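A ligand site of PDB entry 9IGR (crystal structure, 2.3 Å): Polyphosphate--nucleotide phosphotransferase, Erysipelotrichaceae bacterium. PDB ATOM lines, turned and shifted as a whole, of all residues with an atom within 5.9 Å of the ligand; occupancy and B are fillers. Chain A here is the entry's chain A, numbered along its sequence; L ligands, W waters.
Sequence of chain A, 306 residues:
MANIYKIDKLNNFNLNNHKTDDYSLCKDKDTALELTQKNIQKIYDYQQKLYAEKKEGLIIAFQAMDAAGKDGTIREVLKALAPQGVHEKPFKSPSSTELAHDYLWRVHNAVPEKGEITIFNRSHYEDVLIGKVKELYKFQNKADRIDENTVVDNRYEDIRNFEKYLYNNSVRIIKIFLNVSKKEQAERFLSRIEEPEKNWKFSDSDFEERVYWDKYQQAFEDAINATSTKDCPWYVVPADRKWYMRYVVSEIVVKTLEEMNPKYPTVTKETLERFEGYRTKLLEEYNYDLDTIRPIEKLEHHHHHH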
ATOM      1  N   LYS A  29     -25.987   6.576 -17.233  1.00  0.00           N
ATOM      2  CA  LYS A  29     -25.644   7.406 -18.365  1.00  0.00           C
ATOM      3  C   LYS A  29     -26.381   7.043 -19.651  1.00  0.00           C
ATOM      4  O   LYS A  29     -26.752   7.920 -20.409  1.00  0.00           O
ATOM      5  CB  LYS A  29     -24.125   7.235 -18.534  1.00  0.00           C
ATOM      6  CG  LYS A  29     -23.546   7.838 -19.806  1.00  0.00           C
ATOM      7  CD  LYS A  29     -22.055   7.645 -20.069  1.00  0.00           C
ATOM      8  CE  LYS A  29     -21.690   8.315 -21.355  1.00  0.00           C
ATOM      9  NZ  LYS A  29     -20.304   8.765 -21.276  1.00  0.00           N
ATOM     10  N   ALA A  64     -21.835  30.890 -16.595  1.00  0.00           N
ATOM     11  CA  ALA A  64     -20.934  30.007 -15.874  1.00  0.00           C
ATOM     12  C   ALA A  64     -19.499  30.401 -16.127  1.00  0.00           C
ATOM     13  O   ALA A  64     -19.201  31.142 -17.074  1.00  0.00           O
ATOM     14  CB  ALA A  64     -21.190  28.610 -16.384  1.00  0.00           C
ATOM     15  N   MET A  65     -18.614  29.761 -15.378  1.00  0.00           N
ATOM     16  CA  MET A  65     -17.171  29.849 -15.542  1.00  0.00           C
ATOM     17  C   MET A  65     -16.728  29.265 -16.877  1.00  0.00           C
ATOM     18  O   MET A  65     -17.445  28.484 -17.471  1.00  0.00           O
ATOM     19  CB  MET A  65     -16.468  29.138 -14.353  1.00  0.00           C
ATOM     20  CG  MET A  65     -16.815  29.765 -12.957  1.00  0.00           C
ATOM     21  SD  MET A  65     -16.608  31.578 -12.931  1.00  0.00           S
ATOM     22  CE  MET A  65     -14.810  31.420 -12.788  1.00  0.00           C
ATOM     23  N   ASP A  66     -15.521  29.641 -17.333  1.00  0.00           N
ATOM     24  CA  ASP A  66     -14.912  29.061 -18.518  1.00  0.00           C
ATOM     25  C   ASP A  66     -14.764  27.541 -18.367  1.00  0.00           C
ATOM     26  O   ASP A  66     -14.446  27.066 -17.301  1.00  0.00           O
ATOM     27  CB  ASP A  66     -13.575  29.733 -18.827  1.00  0.00           C
ATOM     28  CG  ASP A  66     -13.674  31.225 -19.139  1.00  0.00           C
ATOM     29  OD1 ASP A  66     -14.387  31.576 -20.124  1.00  0.00           O
ATOM     30  OD2 ASP A  66     -13.049  32.040 -18.369  1.00  0.00           O
ATOM     31  N   ALA A  67     -15.115  26.833 -19.429  1.00  0.00           N
ATOM     32  CA  ALA A  67     -15.091  25.383 -19.573  1.00  0.00           C
ATOM     33  C   ALA A  67     -16.065  24.664 -18.650  1.00  0.00           C
ATOM     34  O   ALA A  67     -15.960  23.434 -18.485  1.00  0.00           O
ATOM     35  CB  ALA A  67     -13.678  24.839 -19.428  1.00  0.00           C
ATOM     36  N   ALA A  68     -17.079  25.381 -18.180  1.00  0.00           N
ATOM     37  CA  ALA A  68     -18.151  24.732 -17.463  1.00  0.00           C
ATOM     38  C   ALA A  68     -18.957  23.868 -18.399  1.00  0.00           C
ATOM     39  O   ALA A  68     -19.476  22.890 -17.914  1.00  0.00           O
ATOM     40  CB  ALA A  68     -19.033  25.774 -16.818  1.00  0.00           C
ATOM     41  N   GLY A  69     -19.103  24.271 -19.669  1.00  0.00           N
ATOM     42  CA  GLY A  69     -19.829  23.451 -20.628  1.00  0.00           C
ATOM     43  C   GLY A  69     -20.893  24.212 -21.444  1.00  0.00           C
ATOM     44  O   GLY A  69     -21.805  23.583 -21.993  1.00  0.00           O
ATOM     45  N   LYS A  70     -20.776  25.544 -21.581  1.00  0.00           N
ATOM     46  CA  LYS A  70     -21.831  26.357 -22.206  1.00  0.00           C
ATOM     47  C   LYS A  70     -21.901  26.080 -23.717  1.00  0.00           C
ATOM     48  O   LYS A  70     -22.944  25.661 -24.217  1.00  0.00           O
ATOM     49  CB  LYS A  70     -21.623  27.853 -21.952  1.00  0.00           C
ATOM     50  CG  LYS A  70     -21.547  28.301 -20.494  1.00  0.00           C
ATOM     51  CD  LYS A  70     -21.224  29.767 -20.252  1.00  0.00           C
ATOM     52  CE  LYS A  70     -19.910  30.214 -20.847  1.00  0.00           C
ATOM     53  NZ  LYS A  70     -18.838  29.591 -20.046  1.00  0.00           N
ATOM     54  N   ASP A  71     -20.797  26.250 -24.445  1.00  0.00           N
ATOM     55  CA  ASP A  71     -20.794  25.987 -25.877  1.00  0.00           C
ATOM     56  C   ASP A  71     -21.142  24.521 -26.208  1.00  0.00           C
ATOM     57  O   ASP A  71     -21.834  24.262 -27.167  1.00  0.00           O
ATOM     58  CB  ASP A  71     -19.543  26.497 -26.586  1.00  0.00           C
ATOM     59  CG  ASP A  71     -19.534  28.001 -26.938  1.00  0.00           C
ATOM     60  OD1 ASP A  71     -20.605  28.588 -27.369  1.00  0.00           O
ATOM     61  OD2 ASP A  71     -18.451  28.625 -26.813  1.00  0.00           O
ATOM     62  N   GLY A  72     -20.599  23.539 -25.495  1.00  0.00           N
ATOM     63  CA  GLY A  72     -20.838  22.159 -25.884  1.00  0.00           C
ATOM     64  C   GLY A  72     -22.256  21.732 -25.530  1.00  0.00           C
ATOM     65  O   GLY A  72     -22.859  20.941 -26.264  1.00  0.00           O
ATOM     66  N   THR A  73     -22.829  22.288 -24.455  1.00  0.00           N
ATOM     67  CA  THR A  73     -24.220  22.008 -24.161  1.00  0.00           C
ATOM     68  C   THR A  73     -25.145  22.666 -25.191  1.00  0.00           C
ATOM     69  O   THR A  73     -26.043  22.007 -25.707  1.00  0.00           O
ATOM     70  CB  THR A  73     -24.552  22.451 -22.749  1.00  0.00           C
ATOM     71  OG1 THR A  73     -23.649  21.705 -21.912  1.00  0.00           O
ATOM     72  CG2 THR A  73     -26.025  22.218 -22.426  1.00  0.00           C
ATOM     73  N   ARG A  75     -24.499  23.463 -28.212  1.00  0.00           N
ATOM     74  CA  ARG A  75     -24.348  22.687 -29.434  1.00  0.00           C
ATOM     75  C   ARG A  75     -25.015  21.302 -29.379  1.00  0.00           C
ATOM     76  O   ARG A  75     -25.749  20.933 -30.266  1.00  0.00           O
ATOM     77  CB  ARG A  75     -22.864  22.643 -29.782  1.00  0.00           C
ATOM     78  CG  ARG A  75     -22.706  21.776 -31.019  1.00  0.00           C
ATOM     79  CD  ARG A  75     -21.250  21.876 -31.452  1.00  0.00           C
ATOM     80  NE  ARG A  75     -20.331  21.462 -30.390  1.00  0.00           N
ATOM     81  CZ  ARG A  75     -19.025  21.638 -30.409  1.00  0.00           C
ATOM     82  NH1 ARG A  75     -18.411  22.152 -31.472  1.00  0.00           N
ATOM     83  NH2 ARG A  75     -18.323  21.167 -29.386  1.00  0.00           N
ATOM     84  N   ASN A 121     -25.044  33.104 -24.597  1.00  0.00           N
ATOM     85  CA  ASN A 121     -23.854  32.608 -23.964  1.00  0.00           C
ATOM     86  C   ASN A 121     -23.175  33.703 -23.117  1.00  0.00           C
ATOM     87  O   ASN A 121     -22.528  34.615 -23.625  1.00  0.00           O
ATOM     88  CB  ASN A 121     -22.934  32.086 -25.047  1.00  0.00           C
ATOM     89  CG  ASN A 121     -21.705  31.448 -24.446  1.00  0.00           C
ATOM     90  OD1 ASN A 121     -21.300  31.751 -23.316  1.00  0.00           O
ATOM     91  ND2 ASN A 121     -21.039  30.693 -25.286  1.00  0.00           N
ATOM     92  N   LEU A 178     -24.322  26.648 -14.998  1.00  0.00           N
ATOM     93  CA  LEU A 178     -23.604  25.396 -15.080  1.00  0.00           C
ATOM     94  C   LEU A 178     -22.540  25.447 -13.988  1.00  0.00           C
ATOM     95  O   LEU A 178     -21.566  26.210 -14.061  1.00  0.00           O
ATOM     96  CB  LEU A 178     -22.992  25.184 -16.459  1.00  0.00           C
ATOM     97  CG  LEU A 178     -23.983  25.283 -17.612  1.00  0.00           C
ATOM     98  CD1 LEU A 178     -23.209  25.098 -18.894  1.00  0.00           C
ATOM     99  CD2 LEU A 178     -25.074  24.243 -17.465  1.00  0.00           C
ATOM    100  N   GLU A 184     -12.482  20.178 -12.193  1.00  0.00           N
ATOM    101  CA  GLU A 184     -12.972  19.780 -13.500  1.00  0.00           C
ATOM    102  C   GLU A 184     -12.667  20.815 -14.587  1.00  0.00           C
ATOM    103  O   GLU A 184     -12.370  20.477 -15.718  1.00  0.00           O
ATOM    104  CB  GLU A 184     -14.463  19.437 -13.438  1.00  0.00           C
ATOM    105  CG  GLU A 184     -14.973  18.826 -14.739  1.00  0.00           C
ATOM    106  CD  GLU A 184     -14.379  17.541 -15.279  1.00  0.00           C
ATOM    107  OE1 GLU A 184     -13.751  16.846 -14.464  1.00  0.00           O
ATOM    108  OE2 GLU A 184     -14.527  17.255 -16.527  1.00  0.00           O
ATOM    109  N   ARG A 188     -10.538  20.219 -18.147  1.00  0.00           N
ATOM    110  CA  ARG A 188     -10.966  20.631 -19.472  1.00  0.00           C
ATOM    111  C   ARG A 188     -10.007  21.667 -20.076  1.00  0.00           C
ATOM    112  O   ARG A 188      -9.806  21.650 -21.265  1.00  0.00           O
ATOM    113  CB  ARG A 188     -12.364  21.180 -19.322  1.00  0.00           C
ATOM    114  CG  ARG A 188     -13.381  20.083 -19.110  1.00  0.00           C
ATOM    115  CD  ARG A 188     -14.769  20.632 -18.767  1.00  0.00           C
ATOM    116  NE  ARG A 188     -15.688  19.632 -18.217  1.00  0.00           N
ATOM    117  CZ  ARG A 188     -16.925  19.811 -17.791  1.00  0.00           C
ATOM    118  NH1 ARG A 188     -17.476  21.009 -17.769  1.00  0.00           N
ATOM    119  NH2 ARG A 188     -17.602  18.750 -17.335  1.00  0.00           N
ATOM    120  N   SER A 191      -7.226  19.703 -21.444  1.00  0.00           N
ATOM    121  CA  SER A 191      -7.582  19.080 -22.703  1.00  0.00           C
ATOM    122  C   SER A 191      -7.520  20.134 -23.836  1.00  0.00           C
ATOM    123  O   SER A 191      -6.982  19.848 -24.907  1.00  0.00           O
ATOM    124  CB  SER A 191      -8.891  18.355 -22.568  1.00  0.00           C
ATOM    125  OG  SER A 191      -9.396  17.995 -23.864  1.00  0.00           O
ATOM    126  N   ARG A 192      -7.941  21.383 -23.593  1.00  0.00           N
ATOM    127  CA  ARG A 192      -7.781  22.434 -24.596  1.00  0.00           C
ATOM    128  C   ARG A 192      -6.323  22.717 -24.960  1.00  0.00           C
ATOM    129  O   ARG A 192      -6.018  23.118 -26.057  1.00  0.00           O
ATOM    130  CB  ARG A 192      -8.449  23.725 -24.142  1.00  0.00           C
ATOM    131  CG  ARG A 192      -9.971  23.625 -24.115  1.00  0.00           C
ATOM    132  CD  ARG A 192     -10.510  24.932 -23.535  1.00  0.00           C
ATOM    133  NE  ARG A 192     -11.966  24.923 -23.361  1.00  0.00           N
ATOM    134  CZ  ARG A 192     -12.620  26.038 -23.012  1.00  0.00           C
ATOM    135  NH1 ARG A 192     -11.984  27.111 -22.609  1.00  0.00           N
ATOM    136  NH2 ARG A 192     -13.933  26.089 -22.976  1.00  0.00           N
ATOM    137  N   GLU A 195      -4.841  18.947 -27.038  1.00  0.00           N
ATOM    138  CA  GLU A 195      -5.391  18.596 -28.340  1.00  0.00           C
ATOM    139  C   GLU A 195      -5.259  19.782 -29.307  1.00  0.00           C
ATOM    140  O   GLU A 195      -5.846  20.829 -29.064  1.00  0.00           O
ATOM    141  CB  GLU A 195      -6.890  18.351 -28.241  1.00  0.00           C
ATOM    142  CG  GLU A 195      -7.326  17.691 -26.929  1.00  0.00           C
ATOM    143  CD  GLU A 195      -7.779  16.272 -27.020  1.00  0.00           C
ATOM    144  OE1 GLU A 195      -7.047  15.547 -27.726  1.00  0.00           O
ATOM    145  OE2 GLU A 195      -8.825  15.970 -26.392  1.00  0.00           O
ATOM    146  N   LYS A 198      -8.212  21.924 -30.271  1.00  0.00           N
ATOM    147  CA  LYS A 198      -8.889  22.718 -29.285  1.00  0.00           C
ATOM    148  C   LYS A 198      -8.071  23.928 -28.787  1.00  0.00           C
ATOM    149  O   LYS A 198      -8.503  24.694 -27.921  1.00  0.00           O
ATOM    150  CB  LYS A 198      -9.242  21.790 -28.132  1.00  0.00           C
ATOM    151  CG  LYS A 198     -10.338  20.779 -28.413  1.00  0.00           C
ATOM    152  CD  LYS A 198     -10.719  20.212 -27.027  1.00  0.00           C
ATOM    153  CE  LYS A 198     -11.559  18.998 -26.959  1.00  0.00           C
ATOM    154  NZ  LYS A 198     -11.692  18.694 -25.536  1.00  0.00           N
ATOM    155  N   LYS A 201      -9.311  27.488 -28.382  1.00  0.00           N
ATOM    156  CA  LYS A 201     -10.357  27.784 -27.397  1.00  0.00           C
ATOM    157  C   LYS A 201      -9.770  28.302 -26.091  1.00  0.00           C
ATOM    158  O   LYS A 201     -10.487  28.631 -25.167  1.00  0.00           O
ATOM    159  CB  LYS A 201     -11.141  26.520 -26.993  1.00  0.00           C
ATOM    160  CG  LYS A 201     -11.915  25.920 -28.152  1.00  0.00           C
ATOM    161  CD  LYS A 201     -12.855  24.793 -27.802  1.00  0.00           C
ATOM    162  CE  LYS A 201     -13.857  25.281 -26.860  1.00  0.00           C
ATOM    163  NZ  LYS A 201     -14.839  24.224 -26.625  1.00  0.00           N
ATOM    164  N   ASP A 240     -20.129  18.840 -13.778  1.00  0.00           N
ATOM    165  CA  ASP A 240     -18.955  17.972 -13.821  1.00  0.00           C
ATOM    166  C   ASP A 240     -19.095  16.782 -14.750  1.00  0.00           C
ATOM    167  O   ASP A 240     -18.064  16.321 -15.220  1.00  0.00           O
ATOM    168  CB  ASP A 240     -18.476  17.530 -12.446  1.00  0.00           C
ATOM    169  CG  ASP A 240     -17.818  18.651 -11.615  1.00  0.00           C
ATOM    170  OD1 ASP A 240     -17.600  19.774 -12.092  1.00  0.00           O
ATOM    171  OD2 ASP A 240     -17.585  18.424 -10.427  1.00  0.00           O
ATOM    172  N   ARG A 241     -20.309  16.338 -15.119  1.00  0.00           N
ATOM    173  CA  ARG A 241     -20.404  15.345 -16.169  1.00  0.00           C
ATOM    174  C   ARG A 241     -21.255  15.857 -17.326  1.00  0.00           C
ATOM    175  O   ARG A 241     -22.418  16.250 -17.137  1.00  0.00           O
ATOM    176  CB  ARG A 241     -21.066  14.054 -15.651  1.00  0.00           C
ATOM    177  CG  ARG A 241     -20.865  13.603 -14.211  1.00  0.00           C
ATOM    178  CD  ARG A 241     -21.755  12.453 -13.931  1.00  0.00           C
ATOM    179  NE  ARG A 241     -21.142  11.545 -12.952  1.00  0.00           N
ATOM    180  CZ  ARG A 241     -21.072  11.753 -11.643  1.00  0.00           C
ATOM    181  NH1 ARG A 241     -21.563  12.862 -11.158  1.00  0.00           N
ATOM    182  NH2 ARG A 241     -20.565  10.808 -10.850  1.00  0.00           N
ATOM    183  N   LYS A 242     -20.712  15.780 -18.533  1.00  0.00           N
ATOM    184  CA  LYS A 242     -21.324  16.400 -19.699  1.00  0.00           C
ATOM    185  C   LYS A 242     -22.642  15.696 -20.052  1.00  0.00           C
ATOM    186  O   LYS A 242     -23.617  16.370 -20.303  1.00  0.00           O
ATOM    187  CB  LYS A 242     -20.292  16.473 -20.820  1.00  0.00           C
ATOM    188  CG  LYS A 242     -19.263  17.604 -20.578  1.00  0.00           C
ATOM    189  CD  LYS A 242     -18.107  17.577 -21.575  1.00  0.00           C
ATOM    190  CE  LYS A 242     -17.174  18.773 -21.450  1.00  0.00           C
ATOM    191  NZ  LYS A 242     -16.233  18.739 -22.587  1.00  0.00           N
ATOM    192  N   TRP A 243     -22.686  14.365 -20.070  1.00  0.00           N
ATOM    193  CA  TRP A 243     -23.896  13.647 -20.379  1.00  0.00           C
ATOM    194  C   TRP A 243     -25.019  14.049 -19.428  1.00  0.00           C
ATOM    195  O   TRP A 243     -26.147  14.225 -19.863  1.00  0.00           O
ATOM    196  CB  TRP A 243     -23.620  12.141 -20.358  1.00  0.00           C
ATOM    197  CG  TRP A 243     -23.298  11.543 -19.025  1.00  0.00           C
ATOM    198  CD1 TRP A 243     -22.059  11.170 -18.603  1.00  0.00           C
ATOM    199  CD2 TRP A 243     -24.212  11.123 -17.975  1.00  0.00           C
ATOM    200  NE1 TRP A 243     -22.114  10.638 -17.322  1.00  0.00           N
ATOM    201  CE2 TRP A 243     -23.423  10.571 -16.929  1.00  0.00           C
ATOM    202  CE3 TRP A 243     -25.590  11.167 -17.802  1.00  0.00           C
ATOM    203  CZ2 TRP A 243     -23.969  10.057 -15.770  1.00  0.00           C
ATOM    204  CZ3 TRP A 243     -26.138  10.643 -16.657  1.00  0.00           C
ATOM    205  CH2 TRP A 243     -25.330  10.088 -15.648  1.00  0.00           C
ATOM    206  N   TYR A 244     -24.738  14.213 -18.135  1.00  0.00           N
ATOM    207  CA  TYR A 244     -25.783  14.542 -17.165  1.00  0.00           C
ATOM    208  C   TYR A 244     -26.267  15.974 -17.401  1.00  0.00           C
ATOM    209  O   TYR A 244     -27.456  16.278 -17.373  1.00  0.00           O
ATOM    210  CB  TYR A 244     -25.322  14.339 -15.731  1.00  0.00           C
ATOM    211  CG  TYR A 244     -26.443  14.509 -14.713  1.00  0.00           C
ATOM    212  CD1 TYR A 244     -27.462  13.575 -14.603  1.00  0.00           C
ATOM    213  CD2 TYR A 244     -26.512  15.618 -13.901  1.00  0.00           C
ATOM    214  CE1 TYR A 244     -28.504  13.734 -13.720  1.00  0.00           C
ATOM    215  CE2 TYR A 244     -27.532  15.782 -12.996  1.00  0.00           C
ATOM    216  CZ  TYR A 244     -28.529  14.834 -12.901  1.00  0.00           C
ATOM    217  OH  TYR A 244     -29.551  14.936 -12.009  1.00  0.00           O
ATOM    218  N   ARG A 246     -26.133  17.881 -20.179  1.00  0.00           N
ATOM    219  CA  ARG A 246     -26.974  17.920 -21.378  1.00  0.00           C
ATOM    220  C   ARG A 246     -28.361  17.321 -21.121  1.00  0.00           C
ATOM    221  O   ARG A 246     -29.360  17.866 -21.562  1.00  0.00           O
ATOM    222  CB  ARG A 246     -26.302  17.057 -22.435  1.00  0.00           C
ATOM    223  CG  ARG A 246     -25.007  17.736 -22.849  1.00  0.00           C
ATOM    224  CD  ARG A 246     -24.107  16.865 -23.643  1.00  0.00           C
ATOM    225  NE  ARG A 246     -22.808  17.524 -23.772  1.00  0.00           N
ATOM    226  CZ  ARG A 246     -21.833  17.164 -24.579  1.00  0.00           C
ATOM    227  NH1 ARG A 246     -21.959  16.053 -25.244  1.00  0.00           N
ATOM    228  NH2 ARG A 246     -20.767  17.939 -24.754  1.00  0.00           N
HETATM  229  O1  LIG L   1     -19.106   9.659 -15.526  1.00  0.00           O
HETATM  230  P1  LIG L   1     -18.488   9.922 -17.133  1.00  0.00           P
HETATM  231  O2  LIG L   1     -18.437   8.268 -17.515  1.00  0.00           O
HETATM  232  O3  LIG L   1     -17.879  11.413 -17.758  1.00  0.00           O
HETATM  233  P2  LIG L   1     -18.067  12.717 -18.853  1.00  0.00           P
HETATM  234  O4  LIG L   1     -19.265  12.866 -19.766  1.00  0.00           O
HETATM  235  O5  LIG L   1     -17.103  12.419 -20.140  1.00  0.00           O
HETATM  236  P3  LIG L   1     -17.678  12.074 -21.629  1.00  0.00           P
HETATM  237  O6  LIG L   1     -17.214  10.662 -21.763  1.00  0.00           O
HETATM  238  O7  LIG L   1     -16.895  13.019 -22.669  1.00  0.00           O
HETATM  239  P4  LIG L   1     -16.019  12.615 -23.982  1.00  0.00           P
HETATM  240  O8  LIG L   1     -14.533  12.707 -23.883  1.00  0.00           O
HETATM  241  O9  LIG L   1     -16.395  14.135 -24.298  1.00  0.00           O
HETATM  242  P5  LIG L   1     -15.500  15.461 -24.110  1.00  0.00           P
HETATM  243  O10 LIG L   1     -14.453  15.554 -25.154  1.00  0.00           O
HETATM  244  O11 LIG L   1     -16.383  16.534 -24.942  1.00  0.00           O
HETATM  245  P6  LIG L   1     -16.987  16.564 -26.417  1.00  0.00           P
HETATM  246  O12 LIG L   1     -18.452  16.591 -26.196  1.00  0.00           O
HETATM  247  O13 LIG L   1     -16.616  18.104 -26.737  1.00  0.00           O
HETATM  248  P7  LIG L   1     -17.525  19.347 -26.253  1.00  0.00           P
HETATM  249  O14 LIG L   1     -18.657  19.659 -27.151  1.00  0.00           O
HETATM  250  O15 LIG L   1     -16.338  20.354 -26.586  1.00  0.00           O
HETATM  251  P8  LIG L   1     -15.059  20.762 -25.742  1.00  0.00           P
HETATM  252  O16 LIG L   1     -14.129  21.399 -26.700  1.00  0.00           O
HETATM  253  O17 LIG L   1     -15.624  21.648 -24.590  1.00  0.00           O
HETATM  254  P9  LIG L   1     -14.958  22.314 -23.310  1.00  0.00           P
HETATM  255  O18 LIG L   1     -14.704  21.244 -22.330  1.00  0.00           O
HETATM  256  O19 LIG L   1     -16.314  23.029 -22.977  1.00  0.00           O
HETATM  257  P10 LIG L   1     -17.153  24.208 -23.527  1.00  0.00           P
HETATM  258  O20 LIG L   1     -16.368  24.733 -24.646  1.00  0.00           O
HETATM  259  O21 LIG L   1     -17.070  25.271 -22.347  1.00  0.00           O
HETATM  260  P11 LIG L   1     -17.427  26.822 -22.152  1.00  0.00           P
HETATM  261  O22 LIG L   1     -18.436  27.109 -23.244  1.00  0.00           O
HETATM  262  O23 LIG L   1     -18.338  27.006 -20.963  1.00  0.00           O
HETATM  263  O24 LIG L   1     -16.204  27.636 -21.963  1.00  0.00           O
HETATM  264  O25 LIG L   1     -18.546  23.810 -23.643  1.00  0.00           O
HETATM  265  O26 LIG L   1     -13.881  23.237 -23.773  1.00  0.00           O
HETATM  266  O27 LIG L   1     -14.737  19.579 -24.942  1.00  0.00           O
HETATM  267  O28 LIG L   1     -17.763  19.323 -24.778  1.00  0.00           O
HETATM  268  O29 LIG L   1     -16.385  15.625 -27.408  1.00  0.00           O
HETATM  269  O30 LIG L   1     -15.322  15.856 -22.673  1.00  0.00           O
HETATM  270  O31 LIG L   1     -16.596  11.538 -24.836  1.00  0.00           O
HETATM  271  O32 LIG L   1     -19.133  12.433 -21.806  1.00  0.00           O
HETATM  272  O33 LIG L   1     -17.644  14.106 -18.449  1.00  0.00           O
HETATM  273  O34 LIG L   1     -18.768   9.580 -18.693  1.00  0.00           O
HETATM  274  O   HOH W   1     -15.591  12.827 -27.530  1.00  0.00           O
HETATM  275  O   HOH W   2     -19.307  20.980 -23.064  1.00  0.00           O
HETATM  276  O   HOH W   3     -16.585  30.581 -20.981  1.00  0.00           O
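O20 of the ligand is in salt-bridge range of NZ of Lys 201. The guanidinium group of Arg 192 lies within salt-bridge range of an oxygen (O26) of the ligand (2.6 Å). An oxygen (O14) of the ligand lies within salt-bridge range of the guanidinium group of Arg 75 (2.7 Å). An oxygen (O4) of the ligand is in hydrogen-bond range of the backbone NH of Lys 242 (3.5 Å). NZ of Lys 242 is in salt-bridge range of O28 of the ligand (2.7 Å). An oxygen (O25) of the ligand lies within hydrogen-bond range of the backbone NH of Gly 72 (2.8 Å). O22 of the ligand sits at hydrogen-bond distance from N of Asp 71, 2.8 Å away. The backbone NH of Lys 70 sits at hydrogen-bond distance from an oxygen (O23) of the ligand (2.9 Å). An oxygen (O23) of the ligand is in salt-bridge range of the side-chain amino group (NZ) of Lys 70 (2.8 Å). O24 of the ligand sits at hydrogen-bond distance from N of Ala 67 (2.9 Å). NH2 of Arg 246 is in salt-bridge range of O12 of the ligand. The side-chain amino group (NZ) of Lys 29 is in salt-bridge range of an oxygen (O34) of the ligand (3.1 Å). An oxygen (O23) of the ligand lies within hydrogen-bond range of the backbone NH of Gly 69, 3.1 Å away. O27 of the ligand is in salt-bridge range of NZ of Lys 198 (3.2 Å). The backbone NH (N) of Ala 68 lies within hydrogen-bond range of an oxygen (O23) of the ligand (3.5 Å). O1 of the ligand is in salt-bridge range of NE of Arg 241.
The backbone carbonyl oxygen (O) of Lys 201 sits at hydrogen-bond distance from the guanidinium group (NH1) of Arg 192 (3.3 Å). ND2 of Asn 121 lies within hydrogen-bond range of OD1 of Asp 71 (3.0 Å). NZ of Lys 70 sits at hydrogen-bond distance from O of Met 65. O of Ala 64 is in hydrogen-bond range of NZ of Lys 70 (3.4 Å). The backbone carbonyl oxygen of Ala 67 lies within hydrogen-bond range of the guanidinium group of Arg 188 (2.9 Å). The backbone carbonyl oxygen (O) of Gly 69 is in hydrogen-bond range of the side-chain hydroxyl (OG1) of Thr 73, 2.6 Å away. O of Ala 68 is in hydrogen-bond range of NH1 of Arg 188, at 2.7 Å. O of Asp 240 sits at hydrogen-bond distance from NH2 of Arg 188, at 3.3 Å.
O of Met 65 touches O23 of the ligand, at 3.9 Å. Asp 66 touches the ligand. CD of Arg 188 touches O18 of the ligand, at 3.6 Å. Asp 240 touches the ligand (O to O33, 3.9 Å). Trp 243 touches the ligand. The nearest printed residue that does not touch the ligand is Thr 73 (4.6 Å).
Water W3 lies within hydrogen-bond range of OD1 of Asp 66 (2.6 Å), NZ of Lys 70 (2.6 Å) and O24 of the ligand (3.1 Å).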
